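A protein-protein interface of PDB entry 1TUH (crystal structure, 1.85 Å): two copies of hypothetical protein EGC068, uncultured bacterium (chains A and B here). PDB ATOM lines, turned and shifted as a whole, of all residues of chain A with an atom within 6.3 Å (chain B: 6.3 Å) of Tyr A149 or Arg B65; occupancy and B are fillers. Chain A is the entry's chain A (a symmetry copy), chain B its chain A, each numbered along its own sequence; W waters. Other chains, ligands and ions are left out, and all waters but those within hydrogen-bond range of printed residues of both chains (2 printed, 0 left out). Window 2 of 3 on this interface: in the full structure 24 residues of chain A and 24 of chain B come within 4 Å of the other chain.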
ATOM      1  N   TYR A 146     -15.777 -13.306   8.734  1.00  0.00           N
ATOM      2  CA  TYR A 146     -15.006 -14.502   8.573  1.00  0.00           C
ATOM      3  C   TYR A 146     -13.743 -14.093   7.817  1.00  0.00           C
ATOM      4  O   TYR A 146     -12.703 -14.087   8.385  1.00  0.00           O
ATOM      5  CB  TYR A 146     -15.797 -15.584   7.796  1.00  0.00           C
ATOM      6  CG  TYR A 146     -15.013 -16.888   7.638  1.00  0.00           C
ATOM      7  CD1 TYR A 146     -14.859 -17.780   8.687  1.00  0.00           C
ATOM      8  CD2 TYR A 146     -14.393 -17.207   6.415  1.00  0.00           C
ATOM      9  CE1 TYR A 146     -14.135 -18.924   8.551  1.00  0.00           C
ATOM     10  CE2 TYR A 146     -13.663 -18.369   6.252  1.00  0.00           C
ATOM     11  CZ  TYR A 146     -13.536 -19.236   7.304  1.00  0.00           C
ATOM     12  OH  TYR A 146     -12.830 -20.396   7.191  1.00  0.00           O
ATOM     13  N   ASP A 147     -13.900 -13.672   6.583  1.00  0.00           N
ATOM     14  CA  ASP A 147     -12.693 -13.179   5.805  1.00  0.00           C
ATOM     15  C   ASP A 147     -12.535 -11.646   5.951  1.00  0.00           C
ATOM     16  O   ASP A 147     -13.003 -10.874   5.128  1.00  0.00           O
ATOM     17  CB  ASP A 147     -12.809 -13.621   4.384  1.00  0.00           C
ATOM     18  CG  ASP A 147     -11.546 -13.266   3.571  1.00  0.00           C
ATOM     19  OD1 ASP A 147     -10.603 -12.731   4.161  1.00  0.00           O
ATOM     20  OD2 ASP A 147     -11.467 -13.548   2.377  1.00  0.00           O
ATOM     21  N   LEU A 148     -11.913 -11.247   7.040  1.00  0.00           N
ATOM     22  CA  LEU A 148     -11.726  -9.811   7.363  1.00  0.00           C
ATOM     23  C   LEU A 148     -10.864  -9.147   6.273  1.00  0.00           C
ATOM     24  O   LEU A 148     -11.053  -8.006   5.924  1.00  0.00           O
ATOM     25  CB  LEU A 148     -11.041  -9.696   8.710  1.00  0.00           C
ATOM     26  CG  LEU A 148     -10.798  -8.273   9.249  1.00  0.00           C
ATOM     27  CD1 LEU A 148     -12.077  -7.501   9.255  1.00  0.00           C
ATOM     28  CD2 LEU A 148     -10.135  -8.332  10.566  1.00  0.00           C
ATOM     29  N   TYR A 149      -9.956  -9.927   5.701  1.00  0.00           N
ATOM     30  CA  TYR A 149      -9.104  -9.392   4.604  1.00  0.00           C
ATOM     31  C   TYR A 149      -9.908  -8.957   3.401  1.00  0.00           C
ATOM     32  O   TYR A 149      -9.630  -7.912   2.788  1.00  0.00           O
ATOM     33  CB  TYR A 149      -8.123 -10.456   4.074  1.00  0.00           C
ATOM     34  CG  TYR A 149      -7.019 -10.798   5.002  1.00  0.00           C
ATOM     35  CD1 TYR A 149      -5.768 -10.160   4.914  1.00  0.00           C
ATOM     36  CD2 TYR A 149      -7.179 -11.796   5.947  1.00  0.00           C
ATOM     37  CE1 TYR A 149      -4.739 -10.501   5.773  1.00  0.00           C
ATOM     38  CE2 TYR A 149      -6.186 -12.128   6.793  1.00  0.00           C
ATOM     39  CZ  TYR A 149      -4.959 -11.497   6.709  1.00  0.00           C
ATOM     40  OH  TYR A 149      -3.997 -11.898   7.605  1.00  0.00           O
ATOM     41  N   ALA A 150     -10.914  -9.726   3.016  1.00  0.00           N
ATOM     42  CA  ALA A 150     -11.810  -9.346   1.965  1.00  0.00           C
ATOM     43  C   ALA A 150     -12.553  -8.070   2.238  1.00  0.00           C
ATOM     44  O   ALA A 150     -12.774  -7.215   1.329  1.00  0.00           O
ATOM     45  CB  ALA A 150     -12.819 -10.458   1.648  1.00  0.00           C
ATOM     46  N   TRP A 151     -13.002  -7.924   3.504  1.00  0.00           N
ATOM     47  CA  TRP A 151     -13.706  -6.683   3.854  1.00  0.00           C
ATOM     48  C   TRP A 151     -12.755  -5.511   3.733  1.00  0.00           C
ATOM     49  O   TRP A 151     -13.101  -4.479   3.135  1.00  0.00           O
ATOM     50  CB  TRP A 151     -14.221  -6.826   5.292  1.00  0.00           C
ATOM     51  CG  TRP A 151     -14.686  -5.626   6.017  1.00  0.00           C
ATOM     52  CD1 TRP A 151     -13.979  -4.903   6.880  1.00  0.00           C
ATOM     53  CD2 TRP A 151     -16.001  -5.106   6.033  1.00  0.00           C
ATOM     54  NE1 TRP A 151     -14.757  -3.922   7.446  1.00  0.00           N
ATOM     55  CE2 TRP A 151     -16.010  -4.004   6.925  1.00  0.00           C
ATOM     56  CE3 TRP A 151     -17.183  -5.445   5.385  1.00  0.00           C
ATOM     57  CZ2 TRP A 151     -17.165  -3.266   7.216  1.00  0.00           C
ATOM     58  CZ3 TRP A 151     -18.318  -4.692   5.642  1.00  0.00           C
ATOM     59  CH2 TRP A 151     -18.299  -3.605   6.528  1.00  0.00           C
ATOM     60  N   ASP A 152     -11.582  -5.658   4.301  1.00  0.00           N
ATOM     61  CA  ASP A 152     -10.607  -4.563   4.243  1.00  0.00           C
ATOM     62  C   ASP A 152     -10.169  -4.222   2.818  1.00  0.00           C
ATOM     63  O   ASP A 152     -10.010  -3.020   2.483  1.00  0.00           O
ATOM     64  CB  ASP A 152      -9.402  -4.820   5.090  1.00  0.00           C
ATOM     65  CG  ASP A 152      -9.641  -4.533   6.552  1.00  0.00           C
ATOM     66  OD1 ASP A 152     -10.689  -3.935   6.890  1.00  0.00           O
ATOM     67  OD2 ASP A 152      -8.814  -4.831   7.416  1.00  0.00           O
ATOM     68  N   GLU A 153      -9.939  -5.260   2.027  1.00  0.00           N
ATOM     69  CA  GLU A 153      -9.675  -5.066   0.604  1.00  0.00           C
ATOM     70  C   GLU A 153     -10.760  -4.265  -0.109  1.00  0.00           C
ATOM     71  O   GLU A 153     -10.428  -3.322  -0.828  1.00  0.00           O
ATOM     72  CB  GLU A 153      -9.441  -6.385  -0.107  1.00  0.00           C
ATOM     73  CG  GLU A 153      -9.463  -6.275  -1.637  1.00  0.00           C
ATOM     74  CD  GLU A 153      -8.369  -5.383  -2.228  1.00  0.00           C
ATOM     75  OE1 GLU A 153      -7.283  -5.224  -1.590  1.00  0.00           O
ATOM     76  OE2 GLU A 153      -8.598  -4.867  -3.366  1.00  0.00           O
ATOM     77  N   PHE A 154     -12.044  -4.612   0.069  1.00  0.00           N
ATOM     78  CA  PHE A 154     -13.141  -3.843  -0.516  1.00  0.00           C
ATOM     79  C   PHE A 154     -13.134  -2.350  -0.149  1.00  0.00           C
ATOM     80  O   PHE A 154     -13.532  -1.517  -0.975  1.00  0.00           O
ATOM     81  CB  PHE A 154     -14.494  -4.455  -0.083  1.00  0.00           C
ATOM     82  CG  PHE A 154     -15.712  -3.743  -0.590  1.00  0.00           C
ATOM     83  CD1 PHE A 154     -16.171  -3.966  -1.875  1.00  0.00           C
ATOM     84  CD2 PHE A 154     -16.437  -2.890   0.230  1.00  0.00           C
ATOM     85  CE1 PHE A 154     -17.281  -3.344  -2.361  1.00  0.00           C
ATOM     86  CE2 PHE A 154     -17.581  -2.256  -0.258  1.00  0.00           C
ATOM     87  CZ  PHE A 154     -18.003  -2.494  -1.566  1.00  0.00           C
ATOM     88  N   PRO B  63     -10.409 -19.133   9.344  1.00  0.00           N
ATOM     89  CA  PRO B  63     -10.219 -18.076   8.388  1.00  0.00           C
ATOM     90  C   PRO B  63      -8.740 -17.626   8.393  1.00  0.00           C
ATOM     91  O   PRO B  63      -7.946 -18.009   9.271  1.00  0.00           O
ATOM     92  CB  PRO B  63     -11.131 -16.968   8.877  1.00  0.00           C
ATOM     93  CG  PRO B  63     -11.058 -17.154  10.404  1.00  0.00           C
ATOM     94  CD  PRO B  63     -11.009 -18.648  10.614  1.00  0.00           C
ATOM     95  N   GLY B  64      -8.433 -16.748   7.448  1.00  0.00           N
ATOM     96  CA  GLY B  64      -7.157 -16.053   7.478  1.00  0.00           C
ATOM     97  C   GLY B  64      -6.125 -16.622   6.539  1.00  0.00           C
ATOM     98  O   GLY B  64      -6.432 -17.416   5.663  1.00  0.00           O
ATOM     99  N   ARG B  65      -4.904 -16.170   6.745  1.00  0.00           N
ATOM    100  CA  ARG B  65      -3.843 -16.459   5.785  1.00  0.00           C
ATOM    101  C   ARG B  65      -2.664 -17.167   6.400  1.00  0.00           C
ATOM    102  O   ARG B  65      -1.642 -17.256   5.774  1.00  0.00           O
ATOM    103  CB  ARG B  65      -3.436 -15.154   5.106  1.00  0.00           C
ATOM    104  CG  ARG B  65      -4.448 -14.803   4.011  1.00  0.00           C
ATOM    105  CD  ARG B  65      -4.345 -13.415   3.452  1.00  0.00           C
ATOM    106  NE  ARG B  65      -5.497 -13.116   2.596  1.00  0.00           N
ATOM    107  CZ  ARG B  65      -5.608 -12.027   1.834  1.00  0.00           C
ATOM    108  NH1 ARG B  65      -4.620 -11.148   1.793  1.00  0.00           N
ATOM    109  NH2 ARG B  65      -6.705 -11.820   1.117  1.00  0.00           N
ATOM    110  N   SER B  66      -2.788 -17.692   7.600  1.00  0.00           N
ATOM    111  CA  SER B  66      -1.712 -18.393   8.250  1.00  0.00           C
ATOM    112  C   SER B  66      -1.580 -19.807   7.689  1.00  0.00           C
ATOM    113  O   SER B  66      -2.442 -20.299   6.909  1.00  0.00           O
ATOM    114  CB  SER B  66      -1.974 -18.479   9.771  1.00  0.00           C
ATOM    115  OG  SER B  66      -2.851 -19.567  10.054  1.00  0.00           O
ATOM    116  N   ARG B  67      -0.531 -20.476   8.140  1.00  0.00           N
ATOM    117  CA  ARG B  67      -0.272 -21.852   7.727  1.00  0.00           C
ATOM    118  C   ARG B  67      -1.340 -22.809   8.302  1.00  0.00           C
ATOM    119  O   ARG B  67      -1.492 -23.936   7.807  1.00  0.00           O
ATOM    120  CB  ARG B  67       1.116 -22.314   8.168  1.00  0.00           C
ATOM    121  CG  ARG B  67       1.668 -23.494   7.278  1.00  0.00           C
ATOM    122  CD  ARG B  67       3.216 -23.508   7.077  1.00  0.00           C
ATOM    123  NE  ARG B  67       3.754 -24.822   6.675  1.00  0.00           N
ATOM    124  CZ  ARG B  67       3.646 -25.338   5.450  1.00  0.00           C
ATOM    125  NH1 ARG B  67       2.990 -24.686   4.494  1.00  0.00           N
ATOM    126  NH2 ARG B  67       4.165 -26.511   5.183  1.00  0.00           N
ATOM    127  N   ILE B  68      -2.077 -22.376   9.316  1.00  0.00           N
ATOM    128  CA  ILE B  68      -3.181 -23.238   9.811  1.00  0.00           C
ATOM    129  C   ILE B  68      -4.606 -22.876   9.361  1.00  0.00           C
ATOM    130  O   ILE B  68      -5.569 -23.537   9.777  1.00  0.00           O
ATOM    131  CB  ILE B  68      -3.068 -23.527  11.328  1.00  0.00           C
ATOM    132  CG1 ILE B  68      -3.085 -22.285  12.233  1.00  0.00           C
ATOM    133  CG2 ILE B  68      -1.761 -24.310  11.590  1.00  0.00           C
ATOM    134  CD1 ILE B  68      -4.409 -21.546  12.355  1.00  0.00           C
ATOM    135  N   ALA B  69      -4.724 -21.929   8.435  1.00  0.00           N
ATOM    136  CA  ALA B  69      -5.982 -21.603   7.823  1.00  0.00           C
ATOM    137  C   ALA B  69      -6.536 -22.699   6.944  1.00  0.00           C
ATOM    138  O   ALA B  69      -5.788 -23.519   6.425  1.00  0.00           O
ATOM    139  CB  ALA B  69      -5.846 -20.364   6.990  1.00  0.00           C
ATOM    140  N   LEU B 148      -8.709 -10.768  13.188  1.00  0.00           N
ATOM    141  CA  LEU B 148      -8.118 -11.903  12.436  1.00  0.00           C
ATOM    142  C   LEU B 148      -6.614 -11.650  12.222  1.00  0.00           C
ATOM    143  O   LEU B 148      -5.812 -12.554  12.232  1.00  0.00           O
ATOM    144  CB  LEU B 148      -8.821 -12.025  11.098  1.00  0.00           C
ATOM    145  CG  LEU B 148      -8.380 -13.183  10.183  1.00  0.00           C
ATOM    146  CD1 LEU B 148      -8.454 -14.478  10.922  1.00  0.00           C
ATOM    147  CD2 LEU B 148      -9.161 -13.170   8.931  1.00  0.00           C
ATOM    148  N   TYR B 149      -6.255 -10.379  12.095  1.00  0.00           N
ATOM    149  CA  TYR B 149      -4.819 -10.027  11.930  1.00  0.00           C
ATOM    150  C   TYR B 149      -3.976 -10.448  13.112  1.00  0.00           C
ATOM    151  O   TYR B 149      -2.850 -10.948  12.951  1.00  0.00           O
ATOM    152  CB  TYR B 149      -4.616  -8.504  11.808  1.00  0.00           C
ATOM    153  CG  TYR B 149      -5.087  -7.917  10.531  1.00  0.00           C
ATOM    154  CD1 TYR B 149      -4.211  -7.731   9.445  1.00  0.00           C
ATOM    155  CD2 TYR B 149      -6.396  -7.488  10.395  1.00  0.00           C
ATOM    156  CE1 TYR B 149      -4.658  -7.164   8.266  1.00  0.00           C
ATOM    157  CE2 TYR B 149      -6.842  -6.945   9.248  1.00  0.00           C
ATOM    158  CZ  TYR B 149      -5.981  -6.766   8.180  1.00  0.00           C
ATOM    159  OH  TYR B 149      -6.513  -6.199   7.048  1.00  0.00           O
ATOM    160  N   ASP B 152      -3.529 -14.222  12.888  1.00  0.00           N
ATOM    161  CA  ASP B 152      -2.535 -14.553  11.860  1.00  0.00           C
ATOM    162  C   ASP B 152      -1.109 -14.172  12.257  1.00  0.00           C
ATOM    163  O   ASP B 152      -0.154 -14.942  11.979  1.00  0.00           O
ATOM    164  CB  ASP B 152      -2.862 -13.956  10.529  1.00  0.00           C
ATOM    165  CG  ASP B 152      -3.907 -14.741   9.776  1.00  0.00           C
ATOM    166  OD1 ASP B 152      -4.238 -15.873  10.198  1.00  0.00           O
ATOM    167  OD2 ASP B 152      -4.411 -14.318   8.733  1.00  0.00           O
ATOM    168  N   GLU B 153      -0.975 -12.993  12.849  1.00  0.00           N
ATOM    169  CA  GLU B 153       0.305 -12.588  13.419  1.00  0.00           C
ATOM    170  C   GLU B 153       0.866 -13.592  14.422  1.00  0.00           C
ATOM    171  O   GLU B 153       2.039 -13.952  14.311  1.00  0.00           O
ATOM    172  CB  GLU B 153       0.230 -11.208  14.043  1.00  0.00           C
ATOM    173  CG  GLU B 153       1.440 -10.857  14.919  1.00  0.00           C
ATOM    174  CD  GLU B 153       2.774 -10.808  14.171  1.00  0.00           C
ATOM    175  OE1 GLU B 153       2.783 -10.543  12.929  1.00  0.00           O
ATOM    176  OE2 GLU B 153       3.826 -11.006  14.855  1.00  0.00           O
HETATM  177  O   HOH W   1     -10.450 -15.903   5.595  1.00  0.00           O
HETATM  178  O   HOH W   2      -9.388 -12.777   1.081  1.00  0.00           O
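The backbone nitrogen of Pro B63 lies close to the side-chain hydroxyl of Tyr A146 (3.5 Å).
OD2 of Asp B152 lies within hydrogen-bond range of OH of Tyr A149.
The side-chain hydroxyl (OH) of Tyr B149 is in hydrogen-bond range of the side-chain carboxylate (OD2) of Asp A152, 2.7 Å away.
The backbone NH of Ser B66 sits close to the side-chain carboxylate of Asp B152, 3.5 Å away.
The backbone NH (N) of Arg B65 sits at hydrogen-bond distance from the side-chain carboxylate (OD2) of Asp B152.
The backbone NH (N) of Tyr A149 sits close to the side-chain carboxylate (OD1) of Asp A147 (3.3 Å).
Among the printed residues, pairs that only touch across the chains: Tyr A146 with Leu B148 (3.7 Å), Leu A148 with Leu B148 (3.9 Å), Leu A148 with Tyr B149 (3.8 Å), Tyr A149 with Arg B65 (3.5 Å) and Tyr A149 with Leu B148 (3.8 Å).
Printed residues of chain B within 4 Å of Tyr A149: Arg B65, Leu B148 and Asp B152.
Of the printed residues of chain A, Arg B65 touches Tyr A149.
Of the printed residues of chain A, Leu B148 touches Tyr A146, Leu A148 and Tyr A149.
Printed residues of chain A within 4 Å of Pro B63: Tyr A146.
Of the printed residues of chain B, Tyr A146 touches Pro B63 (3.3 Å) and Leu B148 (3.7 Å).
Ser B66 touches none of the printed residues of chain A.
The nearest printed residue of chain B that does not touch Tyr A149 is Gly B64 (4.1 Å).
The nearest printed residue of chain A that does not touch Arg B65 is Asp A147 (5.0 Å).
Of the 9 printed residues of chain A, 4 touch a printed residue of chain B.
Hydrophobic or aromatic side chains of chain A that line the printed part of chain B: Tyr A146, Leu A148 and Tyr A149.
Of the 11 printed residues of chain B, 5 touch a printed residue of chain A.
Hydrophobic or aromatic side chains of chain B that line the printed part of chain A: Pro B63, Leu B148 and Tyr B149.
Among the printed residues, no Asp or Glu carboxylate lies within 4 Å of a Lys or Arg side-chain nitrogen of the other chain.
Leu A148 touches its own counterpart, Leu B148.
Leu A148 touches Tyr B149, and with the chains exchanged Tyr A149 touches Leu B148.
Tyr A149 touches Asp B152, and with the chains exchanged Asp A152 touches Tyr B149.
4 positions are printed for both chains.
Water W2 lies within hydrogen-bond range of the side-chain carboxylate (OD2) of Asp A147 (2.6 Å) and the guanidinium group (NH2) of Arg B65 (2.8 Å).
Water W1 lies within hydrogen-bond range of the backbone NH (N) of Gly B64 (2.9 Å) and the side-chain carboxylate (OD1) of Asp A147 (3.5 Å).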
